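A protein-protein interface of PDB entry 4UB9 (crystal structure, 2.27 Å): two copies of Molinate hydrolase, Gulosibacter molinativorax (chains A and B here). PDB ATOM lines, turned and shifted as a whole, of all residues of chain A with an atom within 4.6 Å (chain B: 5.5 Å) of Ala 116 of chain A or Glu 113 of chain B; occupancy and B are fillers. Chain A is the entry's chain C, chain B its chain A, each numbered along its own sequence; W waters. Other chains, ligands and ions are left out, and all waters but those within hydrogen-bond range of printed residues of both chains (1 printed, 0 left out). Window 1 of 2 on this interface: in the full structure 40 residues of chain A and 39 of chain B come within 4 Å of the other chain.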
ATOM      1  N   ILE A 112      25.322  -8.995 -18.281  1.00  0.00           N
ATOM      2  CA  ILE A 112      24.958 -10.262 -17.651  1.00  0.00           C
ATOM      3  C   ILE A 112      24.047 -10.019 -16.487  1.00  0.00           C
ATOM      4  O   ILE A 112      22.968 -10.590 -16.410  1.00  0.00           O
ATOM      5  CB  ILE A 112      26.178 -11.044 -17.164  1.00  0.00           C
ATOM      6  CG1 ILE A 112      27.078 -11.433 -18.341  1.00  0.00           C
ATOM      7  CG2 ILE A 112      25.750 -12.304 -16.436  1.00  0.00           C
ATOM      8  CD1 ILE A 112      28.448 -11.906 -17.906  1.00  0.00           C
ATOM      9  N   GLU A 113      24.493  -9.170 -15.578  1.00  0.00           N
ATOM     10  CA  GLU A 113      23.772  -8.926 -14.355  1.00  0.00           C
ATOM     11  C   GLU A 113      22.378  -8.383 -14.625  1.00  0.00           C
ATOM     12  O   GLU A 113      21.401  -8.799 -13.997  1.00  0.00           O
ATOM     13  CB  GLU A 113      24.550  -8.019 -13.369  1.00  0.00           C
ATOM     14  CG  GLU A 113      24.904  -6.636 -13.885  1.00  0.00           C
ATOM     15  CD  GLU A 113      26.092  -5.981 -13.147  1.00  0.00           C
ATOM     16  OE1 GLU A 113      25.863  -5.276 -12.122  1.00  0.00           O
ATOM     17  OE2 GLU A 113      27.227  -6.134 -13.625  1.00  0.00           O
ATOM     18  N   TYR A 114      22.284  -7.460 -15.560  1.00  0.00           N
ATOM     19  CA  TYR A 114      21.000  -6.860 -15.887  1.00  0.00           C
ATOM     20  C   TYR A 114      20.044  -7.882 -16.498  1.00  0.00           C
ATOM     21  O   TYR A 114      18.890  -7.985 -16.076  1.00  0.00           O
ATOM     22  CB  TYR A 114      21.258  -5.732 -16.862  1.00  0.00           C
ATOM     23  CG  TYR A 114      20.116  -4.979 -17.489  1.00  0.00           C
ATOM     24  CD1 TYR A 114      19.457  -3.964 -16.803  1.00  0.00           C
ATOM     25  CD2 TYR A 114      19.796  -5.179 -18.819  1.00  0.00           C
ATOM     26  CE1 TYR A 114      18.473  -3.197 -17.439  1.00  0.00           C
ATOM     27  CE2 TYR A 114      18.822  -4.429 -19.451  1.00  0.00           C
ATOM     28  CZ  TYR A 114      18.165  -3.436 -18.761  1.00  0.00           C
ATOM     29  OH  TYR A 114      17.202  -2.704 -19.411  1.00  0.00           O
ATOM     30  N   LEU A 115      20.497  -8.606 -17.503  1.00  0.00           N
ATOM     31  CA  LEU A 115      19.588  -9.549 -18.163  1.00  0.00           C
ATOM     32  C   LEU A 115      19.197 -10.692 -17.267  1.00  0.00           C
ATOM     33  O   LEU A 115      18.073 -11.217 -17.347  1.00  0.00           O
ATOM     34  CB  LEU A 115      20.167 -10.080 -19.464  1.00  0.00           C
ATOM     35  CG  LEU A 115      20.257  -8.992 -20.532  1.00  0.00           C
ATOM     36  CD1 LEU A 115      21.027  -9.453 -21.763  1.00  0.00           C
ATOM     37  CD2 LEU A 115      18.856  -8.518 -20.931  1.00  0.00           C
ATOM     38  N   ALA A 116      20.108 -11.091 -16.381  1.00  0.00           N
ATOM     39  CA  ALA A 116      19.776 -12.178 -15.469  1.00  0.00           C
ATOM     40  C   ALA A 116      18.807 -11.689 -14.390  1.00  0.00           C
ATOM     41  O   ALA A 116      17.865 -12.378 -13.985  1.00  0.00           O
ATOM     42  CB  ALA A 116      21.022 -12.769 -14.850  1.00  0.00           C
ATOM     43  N   ARG A 117      19.051 -10.491 -13.917  1.00  0.00           N
ATOM     44  CA  ARG A 117      18.230  -9.976 -12.834  1.00  0.00           C
ATOM     45  C   ARG A 117      16.755  -9.791 -13.244  1.00  0.00           C
ATOM     46  O   ARG A 117      15.880  -9.995 -12.466  1.00  0.00           O
ATOM     47  CB  ARG A 117      18.776  -8.643 -12.345  1.00  0.00           C
ATOM     48  CG  ARG A 117      18.168  -8.182 -11.030  1.00  0.00           C
ATOM     49  CD  ARG A 117      18.710  -6.790 -10.690  1.00  0.00           C
ATOM     50  NE  ARG A 117      20.174  -6.779 -10.508  1.00  0.00           N
ATOM     51  CZ  ARG A 117      20.780  -7.077  -9.355  1.00  0.00           C
ATOM     52  NH1 ARG A 117      20.065  -7.443  -8.291  1.00  0.00           N
ATOM     53  NH2 ARG A 117      22.098  -6.996  -9.252  1.00  0.00           N
ATOM     54  N   PHE A 118      16.530  -9.398 -14.474  1.00  0.00           N
ATOM     55  CA  PHE A 118      15.180  -9.098 -14.904  1.00  0.00           C
ATOM     56  C   PHE A 118      14.503 -10.125 -15.817  1.00  0.00           C
ATOM     57  O   PHE A 118      13.413  -9.887 -16.260  1.00  0.00           O
ATOM     58  CB  PHE A 118      15.153  -7.707 -15.521  1.00  0.00           C
ATOM     59  CG  PHE A 118      15.582  -6.687 -14.562  1.00  0.00           C
ATOM     60  CD1 PHE A 118      14.842  -6.472 -13.406  1.00  0.00           C
ATOM     61  CD2 PHE A 118      16.763  -6.029 -14.731  1.00  0.00           C
ATOM     62  CE1 PHE A 118      15.243  -5.568 -12.467  1.00  0.00           C
ATOM     63  CE2 PHE A 118      17.194  -5.142 -13.771  1.00  0.00           C
ATOM     64  CZ  PHE A 118      16.434  -4.901 -12.638  1.00  0.00           C
ATOM     65  N   GLU A 119      15.152 -11.262 -16.057  1.00  0.00           N
ATOM     66  CA  GLU A 119      14.552 -12.328 -16.855  1.00  0.00           C
ATOM     67  C   GLU A 119      13.198 -12.673 -16.238  1.00  0.00           C
ATOM     68  O   GLU A 119      13.112 -12.878 -15.059  1.00  0.00           O
ATOM     69  CB  GLU A 119      15.410 -13.606 -16.943  1.00  0.00           C
ATOM     70  CG  GLU A 119      14.907 -14.564 -18.030  1.00  0.00           C
ATOM     71  CD  GLU A 119      15.895 -15.628 -18.471  1.00  0.00           C
ATOM     72  OE1 GLU A 119      16.771 -16.026 -17.667  1.00  0.00           O
ATOM     73  OE2 GLU A 119      15.786 -16.124 -19.623  1.00  0.00           O
ATOM     74  N   VAL A 195      32.681 -15.842 -18.936  1.00  0.00           N
ATOM     75  CA  VAL A 195      32.327 -16.005 -17.527  1.00  0.00           C
ATOM     76  C   VAL A 195      30.868 -16.248 -17.245  1.00  0.00           C
ATOM     77  O   VAL A 195      30.418 -16.146 -16.110  1.00  0.00           O
ATOM     78  CB  VAL A 195      32.751 -14.775 -16.709  1.00  0.00           C
ATOM     79  CG1 VAL A 195      34.226 -14.535 -16.827  1.00  0.00           C
ATOM     80  CG2 VAL A 195      32.032 -13.515 -17.158  1.00  0.00           C
ATOM     81  N   MET A 196      30.107 -16.547 -18.282  1.00  0.00           N
ATOM     82  CA  MET A 196      28.660 -16.853 -18.124  1.00  0.00           C
ATOM     83  C   MET A 196      28.373 -18.177 -18.782  1.00  0.00           C
ATOM     84  O   MET A 196      29.204 -18.680 -19.546  1.00  0.00           O
ATOM     85  CB  MET A 196      27.816 -15.756 -18.772  1.00  0.00           C
ATOM     86  CG  MET A 196      27.917 -15.744 -20.282  1.00  0.00           C
ATOM     87  SD  MET A 196      27.259 -14.264 -21.058  1.00  0.00           S
ATOM     88  CE  MET A 196      25.548 -14.416 -20.545  1.00  0.00           C
ATOM     89  N   SER A 197      27.229 -18.769 -18.470  1.00  0.00           N
ATOM     90  CA  SER A 197      26.848 -20.022 -19.095  1.00  0.00           C
ATOM     91  C   SER A 197      26.554 -19.808 -20.542  1.00  0.00           C
ATOM     92  O   SER A 197      26.038 -18.767 -20.958  1.00  0.00           O
ATOM     93  CB  SER A 197      25.619 -20.643 -18.450  1.00  0.00           C
ATOM     94  OG  SER A 197      24.489 -19.816 -18.577  1.00  0.00           O
ATOM     95  N   PHE A 200      22.739 -19.591 -21.195  1.00  0.00           N
ATOM     96  CA  PHE A 200      22.101 -18.307 -20.913  1.00  0.00           C
ATOM     97  C   PHE A 200      22.459 -17.344 -21.972  1.00  0.00           C
ATOM     98  O   PHE A 200      21.616 -16.634 -22.488  1.00  0.00           O
ATOM     99  CB  PHE A 200      22.507 -17.737 -19.555  1.00  0.00           C
ATOM    100  CG  PHE A 200      21.851 -16.405 -19.226  1.00  0.00           C
ATOM    101  CD1 PHE A 200      20.489 -16.246 -19.295  1.00  0.00           C
ATOM    102  CD2 PHE A 200      22.609 -15.338 -18.838  1.00  0.00           C
ATOM    103  CE1 PHE A 200      19.900 -15.030 -18.985  1.00  0.00           C
ATOM    104  CE2 PHE A 200      22.036 -14.130 -18.518  1.00  0.00           C
ATOM    105  CZ  PHE A 200      20.680 -13.973 -18.579  1.00  0.00           C
ATOM    106  N   ARG B 109      32.415 -20.305 -14.461  1.00  0.00           N
ATOM    107  CA  ARG B 109      31.346 -19.504 -15.036  1.00  0.00           C
ATOM    108  C   ARG B 109      30.117 -19.513 -14.156  1.00  0.00           C
ATOM    109  O   ARG B 109      29.855 -20.497 -13.498  1.00  0.00           O
ATOM    110  CB  ARG B 109      30.897 -20.062 -16.366  1.00  0.00           C
ATOM    111  CG  ARG B 109      31.990 -20.309 -17.337  1.00  0.00           C
ATOM    112  CD  ARG B 109      31.539 -21.147 -18.534  1.00  0.00           C
ATOM    113  NE  ARG B 109      32.669 -21.224 -19.435  1.00  0.00           N
ATOM    114  CZ  ARG B 109      32.895 -20.340 -20.399  1.00  0.00           C
ATOM    115  NH1 ARG B 109      32.028 -19.359 -20.624  1.00  0.00           N
ATOM    116  NH2 ARG B 109      34.006 -20.416 -21.143  1.00  0.00           N
ATOM    117  N   GLY B 110      29.348 -18.434 -14.204  1.00  0.00           N
ATOM    118  CA  GLY B 110      28.006 -18.439 -13.615  1.00  0.00           C
ATOM    119  C   GLY B 110      27.782 -17.530 -12.432  1.00  0.00           C
ATOM    120  O   GLY B 110      26.625 -17.268 -12.053  1.00  0.00           O
ATOM    121  N   GLY B 111      28.866 -17.116 -11.789  1.00  0.00           N
ATOM    122  CA  GLY B 111      28.765 -16.312 -10.551  1.00  0.00           C
ATOM    123  C   GLY B 111      27.901 -15.072 -10.704  1.00  0.00           C
ATOM    124  O   GLY B 111      27.058 -14.768  -9.861  1.00  0.00           O
ATOM    125  N   ILE B 112      28.100 -14.355 -11.805  1.00  0.00           N
ATOM    126  CA  ILE B 112      27.415 -13.099 -11.986  1.00  0.00           C
ATOM    127  C   ILE B 112      25.927 -13.356 -12.126  1.00  0.00           C
ATOM    128  O   ILE B 112      25.125 -12.770 -11.399  1.00  0.00           O
ATOM    129  CB  ILE B 112      27.893 -12.328 -13.189  1.00  0.00           C
ATOM    130  CG1 ILE B 112      29.358 -11.921 -13.033  1.00  0.00           C
ATOM    131  CG2 ILE B 112      27.068 -11.045 -13.348  1.00  0.00           C
ATOM    132  CD1 ILE B 112      29.976 -11.435 -14.316  1.00  0.00           C
ATOM    133  N   GLU B 113      25.584 -14.211 -13.080  1.00  0.00           N
ATOM    134  CA  GLU B 113      24.183 -14.454 -13.433  1.00  0.00           C
ATOM    135  C   GLU B 113      23.420 -15.027 -12.264  1.00  0.00           C
ATOM    136  O   GLU B 113      22.322 -14.577 -11.937  1.00  0.00           O
ATOM    137  CB  GLU B 113      24.021 -15.344 -14.674  1.00  0.00           C
ATOM    138  CG  GLU B 113      24.633 -16.735 -14.564  1.00  0.00           C
ATOM    139  CD  GLU B 113      24.919 -17.367 -15.922  1.00  0.00           C
ATOM    140  OE1 GLU B 113      24.026 -18.072 -16.473  1.00  0.00           O
ATOM    141  OE2 GLU B 113      26.064 -17.220 -16.419  1.00  0.00           O
ATOM    142  N   TYR B 114      24.043 -15.938 -11.552  1.00  0.00           N
ATOM    143  CA  TYR B 114      23.404 -16.534 -10.371  1.00  0.00           C
ATOM    144  C   TYR B 114      23.175 -15.516  -9.238  1.00  0.00           C
ATOM    145  O   TYR B 114      22.081 -15.405  -8.685  1.00  0.00           O
ATOM    146  CB  TYR B 114      24.300 -17.646  -9.900  1.00  0.00           C
ATOM    147  CG  TYR B 114      23.972 -18.405  -8.624  1.00  0.00           C
ATOM    148  CD1 TYR B 114      23.017 -19.444  -8.614  1.00  0.00           C
ATOM    149  CD2 TYR B 114      24.696 -18.202  -7.473  1.00  0.00           C
ATOM    150  CE1 TYR B 114      22.786 -20.203  -7.478  1.00  0.00           C
ATOM    151  CE2 TYR B 114      24.474 -18.976  -6.322  1.00  0.00           C
ATOM    152  CZ  TYR B 114      23.509 -19.948  -6.333  1.00  0.00           C
ATOM    153  OH  TYR B 114      23.314 -20.688  -5.203  1.00  0.00           O
ATOM    154  N   LEU B 115      24.207 -14.764  -8.887  1.00  0.00           N
ATOM    155  CA  LEU B 115      24.038 -13.830  -7.761  1.00  0.00           C
ATOM    156  C   LEU B 115      23.095 -12.676  -8.103  1.00  0.00           C
ATOM    157  O   LEU B 115      22.413 -12.147  -7.223  1.00  0.00           O
ATOM    158  CB  LEU B 115      25.381 -13.309  -7.270  1.00  0.00           C
ATOM    159  CG  LEU B 115      26.224 -14.412  -6.577  1.00  0.00           C
ATOM    160  CD1 LEU B 115      27.645 -13.941  -6.281  1.00  0.00           C
ATOM    161  CD2 LEU B 115      25.574 -14.858  -5.298  1.00  0.00           C
ATOM    162  N   ALA B 116      23.097 -12.260  -9.359  1.00  0.00           N
ATOM    163  CA  ALA B 116      22.220 -11.169  -9.749  1.00  0.00           C
ATOM    164  C   ALA B 116      20.790 -11.668  -9.805  1.00  0.00           C
ATOM    165  O   ALA B 116      19.841 -10.988  -9.399  1.00  0.00           O
ATOM    166  CB  ALA B 116      22.634 -10.587 -11.075  1.00  0.00           C
ATOM    167  N   ARG B 117      20.634 -12.876 -10.296  1.00  0.00           N
ATOM    168  CA  ARG B 117      19.289 -13.387 -10.473  1.00  0.00           C
ATOM    169  C   ARG B 117      18.592 -13.535  -9.151  1.00  0.00           C
ATOM    170  O   ARG B 117      17.403 -13.343  -9.052  1.00  0.00           O
ATOM    171  CB  ARG B 117      19.314 -14.728 -11.216  1.00  0.00           C
ATOM    172  CG  ARG B 117      17.938 -15.207 -11.706  1.00  0.00           C
ATOM    173  CD  ARG B 117      18.037 -16.604 -12.322  1.00  0.00           C
ATOM    174  NE  ARG B 117      18.877 -16.678 -13.500  1.00  0.00           N
ATOM    175  CZ  ARG B 117      18.485 -16.318 -14.721  1.00  0.00           C
ATOM    176  NH1 ARG B 117      17.268 -15.856 -14.929  1.00  0.00           N
ATOM    177  NH2 ARG B 117      19.339 -16.401 -15.750  1.00  0.00           N
ATOM    178  N   PHE B 118      19.330 -13.939  -8.121  1.00  0.00           N
ATOM    179  CA  PHE B 118      18.680 -14.248  -6.835  1.00  0.00           C
ATOM    180  C   PHE B 118      18.855 -13.232  -5.731  1.00  0.00           C
ATOM    181  O   PHE B 118      18.406 -13.473  -4.627  1.00  0.00           O
ATOM    182  CB  PHE B 118      19.081 -15.638  -6.382  1.00  0.00           C
ATOM    183  CG  PHE B 118      18.685 -16.678  -7.379  1.00  0.00           C
ATOM    184  CD1 PHE B 118      17.345 -16.898  -7.648  1.00  0.00           C
ATOM    185  CD2 PHE B 118      19.625 -17.332  -8.135  1.00  0.00           C
ATOM    186  CE1 PHE B 118      16.946 -17.805  -8.616  1.00  0.00           C
ATOM    187  CE2 PHE B 118      19.241 -18.245  -9.117  1.00  0.00           C
ATOM    188  CZ  PHE B 118      17.891 -18.476  -9.351  1.00  0.00           C
ATOM    189  N   ASP B 378      23.269 -23.946 -10.691  1.00  0.00           N
ATOM    190  CA  ASP B 378      22.264 -23.304 -11.533  1.00  0.00           C
ATOM    191  C   ASP B 378      21.988 -24.161 -12.769  1.00  0.00           C
ATOM    192  O   ASP B 378      22.929 -24.585 -13.449  1.00  0.00           O
ATOM    193  CB  ASP B 378      22.730 -21.912 -11.962  1.00  0.00           C
ATOM    194  CG  ASP B 378      21.620 -21.089 -12.585  1.00  0.00           C
ATOM    195  OD1 ASP B 378      21.395 -21.233 -13.806  1.00  0.00           O
ATOM    196  OD2 ASP B 378      21.001 -20.281 -11.871  1.00  0.00           O
ATOM    197  N   ASP B 380      21.057 -23.411 -15.754  1.00  0.00           N
ATOM    198  CA  ASP B 380      21.717 -22.922 -16.987  1.00  0.00           C
ATOM    199  C   ASP B 380      23.146 -23.423 -17.107  1.00  0.00           C
ATOM    200  O   ASP B 380      23.640 -23.682 -18.213  1.00  0.00           O
ATOM    201  CB  ASP B 380      21.720 -21.394 -17.112  1.00  0.00           C
ATOM    202  CG  ASP B 380      20.426 -20.838 -17.604  1.00  0.00           C
ATOM    203  OD1 ASP B 380      19.677 -21.529 -18.328  1.00  0.00           O
ATOM    204  OD2 ASP B 380      20.163 -19.665 -17.295  1.00  0.00           O
ATOM    205  N   ILE B 381      23.824 -23.536 -15.977  1.00  0.00           N
ATOM    206  CA  ILE B 381      25.220 -24.036 -15.958  1.00  0.00           C
ATOM    207  C   ILE B 381      25.276 -25.552 -16.127  1.00  0.00           C
ATOM    208  O   ILE B 381      26.143 -26.082 -16.814  1.00  0.00           O
ATOM    209  CB  ILE B 381      25.935 -23.641 -14.649  1.00  0.00           C
ATOM    210  CG1 ILE B 381      26.133 -22.122 -14.591  1.00  0.00           C
ATOM    211  CG2 ILE B 381      27.282 -24.349 -14.483  1.00  0.00           C
ATOM    212  CD1 ILE B 381      27.297 -21.648 -15.430  1.00  0.00           C
HETATM  213  O   HOH W   1      27.476 -15.353 -15.009  1.00  0.00           O
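Water W1 lies within hydrogen-bond range of the side-chain carboxylate of Glu 113 of chain B (2.7 Å), the backbone carbonyl oxygen of Val 195 of chain A (3.2 Å) and the backbone NH of Ile 112 of chain B (3.4 Å).
The backbone carbonyl oxygen of Met 196 of chain A lies within hydrogen-bond range of the guanidinium group of Arg 109 of chain B.
The backbone NH of Gly 110 of chain B is in hydrogen-bond range of the backbone carbonyl oxygen of Val 195 of chain A, 3.2 Å away.
The side-chain hydroxyl (OG) of Ser 197 of chain A is in hydrogen-bond range of the side-chain carboxylate (OE1) of Glu 113 of chain B, 2.8 Å away.
The guanidinium group (NH1) of Arg 117 of chain B lies within salt-bridge range of the side-chain carboxylate (OE1) of Glu 119 of chain A, 2.8 Å away.
Hydrophobic or aromatic side chains of chain A within 4 Å of the printed part of chain B: Ile 112, Ala 116, Met 196 and Phe 200.
Of the 13 printed residues of chain B, 8 touch a printed residue of chain A.
Printed residues of chain B that touch a printed residue of chain A: Arg 109, Gly 110, Ile 112, Glu 113, Ala 116, Arg 117, Asp 380 and Ile 381.
Along chain B the printed residues that touch a printed residue of chain A span positions 109 to 381.
Among the printed residues, 18 pairs touch across the chains.
Among the printed residues, Asp or Glu carboxylates within 4 Å of a Lys or Arg side-chain nitrogen of the other chain: Glu 119 of chain A with Arg 117 of chain B.
Printed residues of chain B within 4 Å of Ile 112 of chain A: Ile 112 and Glu 113.
Ala 116 of chain A touches two residues of chain B.
Of the printed residues of chain B, Phe 200 of chain A touches Glu 113 (3.5 Å), Arg 117 (3.6 Å) and Asp 380 (3.8 Å).
Of the printed residues of chain A, Glu 113 of chain B touches Ile 112 (3.9 Å), Ala 116 (3.7 Å), Met 196 (3.1 Å), Ser 197 (2.8 Å) and Phe 200 (3.5 Å).
Printed residues of chain A within 4 Å of Ala 116 of chain B: Glu 113 (3.6 Å) and Arg 117 (3.7 Å).
Printed residues of chain A within 4 Å of Ile 381 of chain B: Ser 197.
Among the printed residues, pairs that only touch across the chains: Met 196 of chain A with Glu 113 of chain B (3.1 Å), Phe 200 of chain A with Glu 113 of chain B (3.5 Å), Ser 197 of chain A with Asp 380 of chain B (3.5 Å), Phe 200 of chain A with Arg 117 of chain B (3.6 Å), Ile 112 of chain A with Ile 112 of chain B (3.6 Å), Ser 197 of chain A with Ile 381 of chain B (3.6 Å), Ala 116 of chain A with Arg 117 of chain B (3.6 Å), Glu 113 of chain A with Ala 116 of chain B (3.6 Å), Val 195 of chain A with Arg 109 of chain B (3.6 Å), Arg 117 of chain A with Ala 116 of chain B (3.7 Å), Ala 116 of chain A with Glu 113 of chain B (3.7 Å), Phe 200 of chain A with Asp 380 of chain B (3.8 Å), Ile 112 of chain A with Glu 113 of chain B (3.9 Å) and Glu 113 of chain A with Ile 112 of chain B (3.9 Å).
Ile 112 of chain A touches its own counterpart, Ile 112 of chain B.
Ile 112 of chain A touches Glu 113 of chain B, and with the chains exchanged Glu 113 of chain A touches Ile 112 of chain B.
Glu 113 of chain A touches Ala 116 of chain B, and with the chains exchanged Ala 116 of chain A touches Glu 113 of chain B.
Ala 116 of chain A touches Arg 117 of chain B, and with the chains exchanged Arg 117 of chain A touches Ala 116 of chain B.
Positions printed for both chains: 112, 113, 114, 115, 116, 117 and 118.
Of the 18 pairs that touch across the chains among the printed residues, 7 have their exchanged pair printed and touching as well.
NH2 of Arg 117 of chain B lies within salt-bridge range of OD2 of Asp 380 of chain B (3.7 Å).
OD1 of Asp 378 of chain B sits at hydrogen-bond distance from N of Asp 380 of chain B, at 2.9 Å.
The backbone NH (N) of Phe 200 of chain A sits close to the side-chain hydroxyl (OG) of Ser 197 of chain A (3.2 Å).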
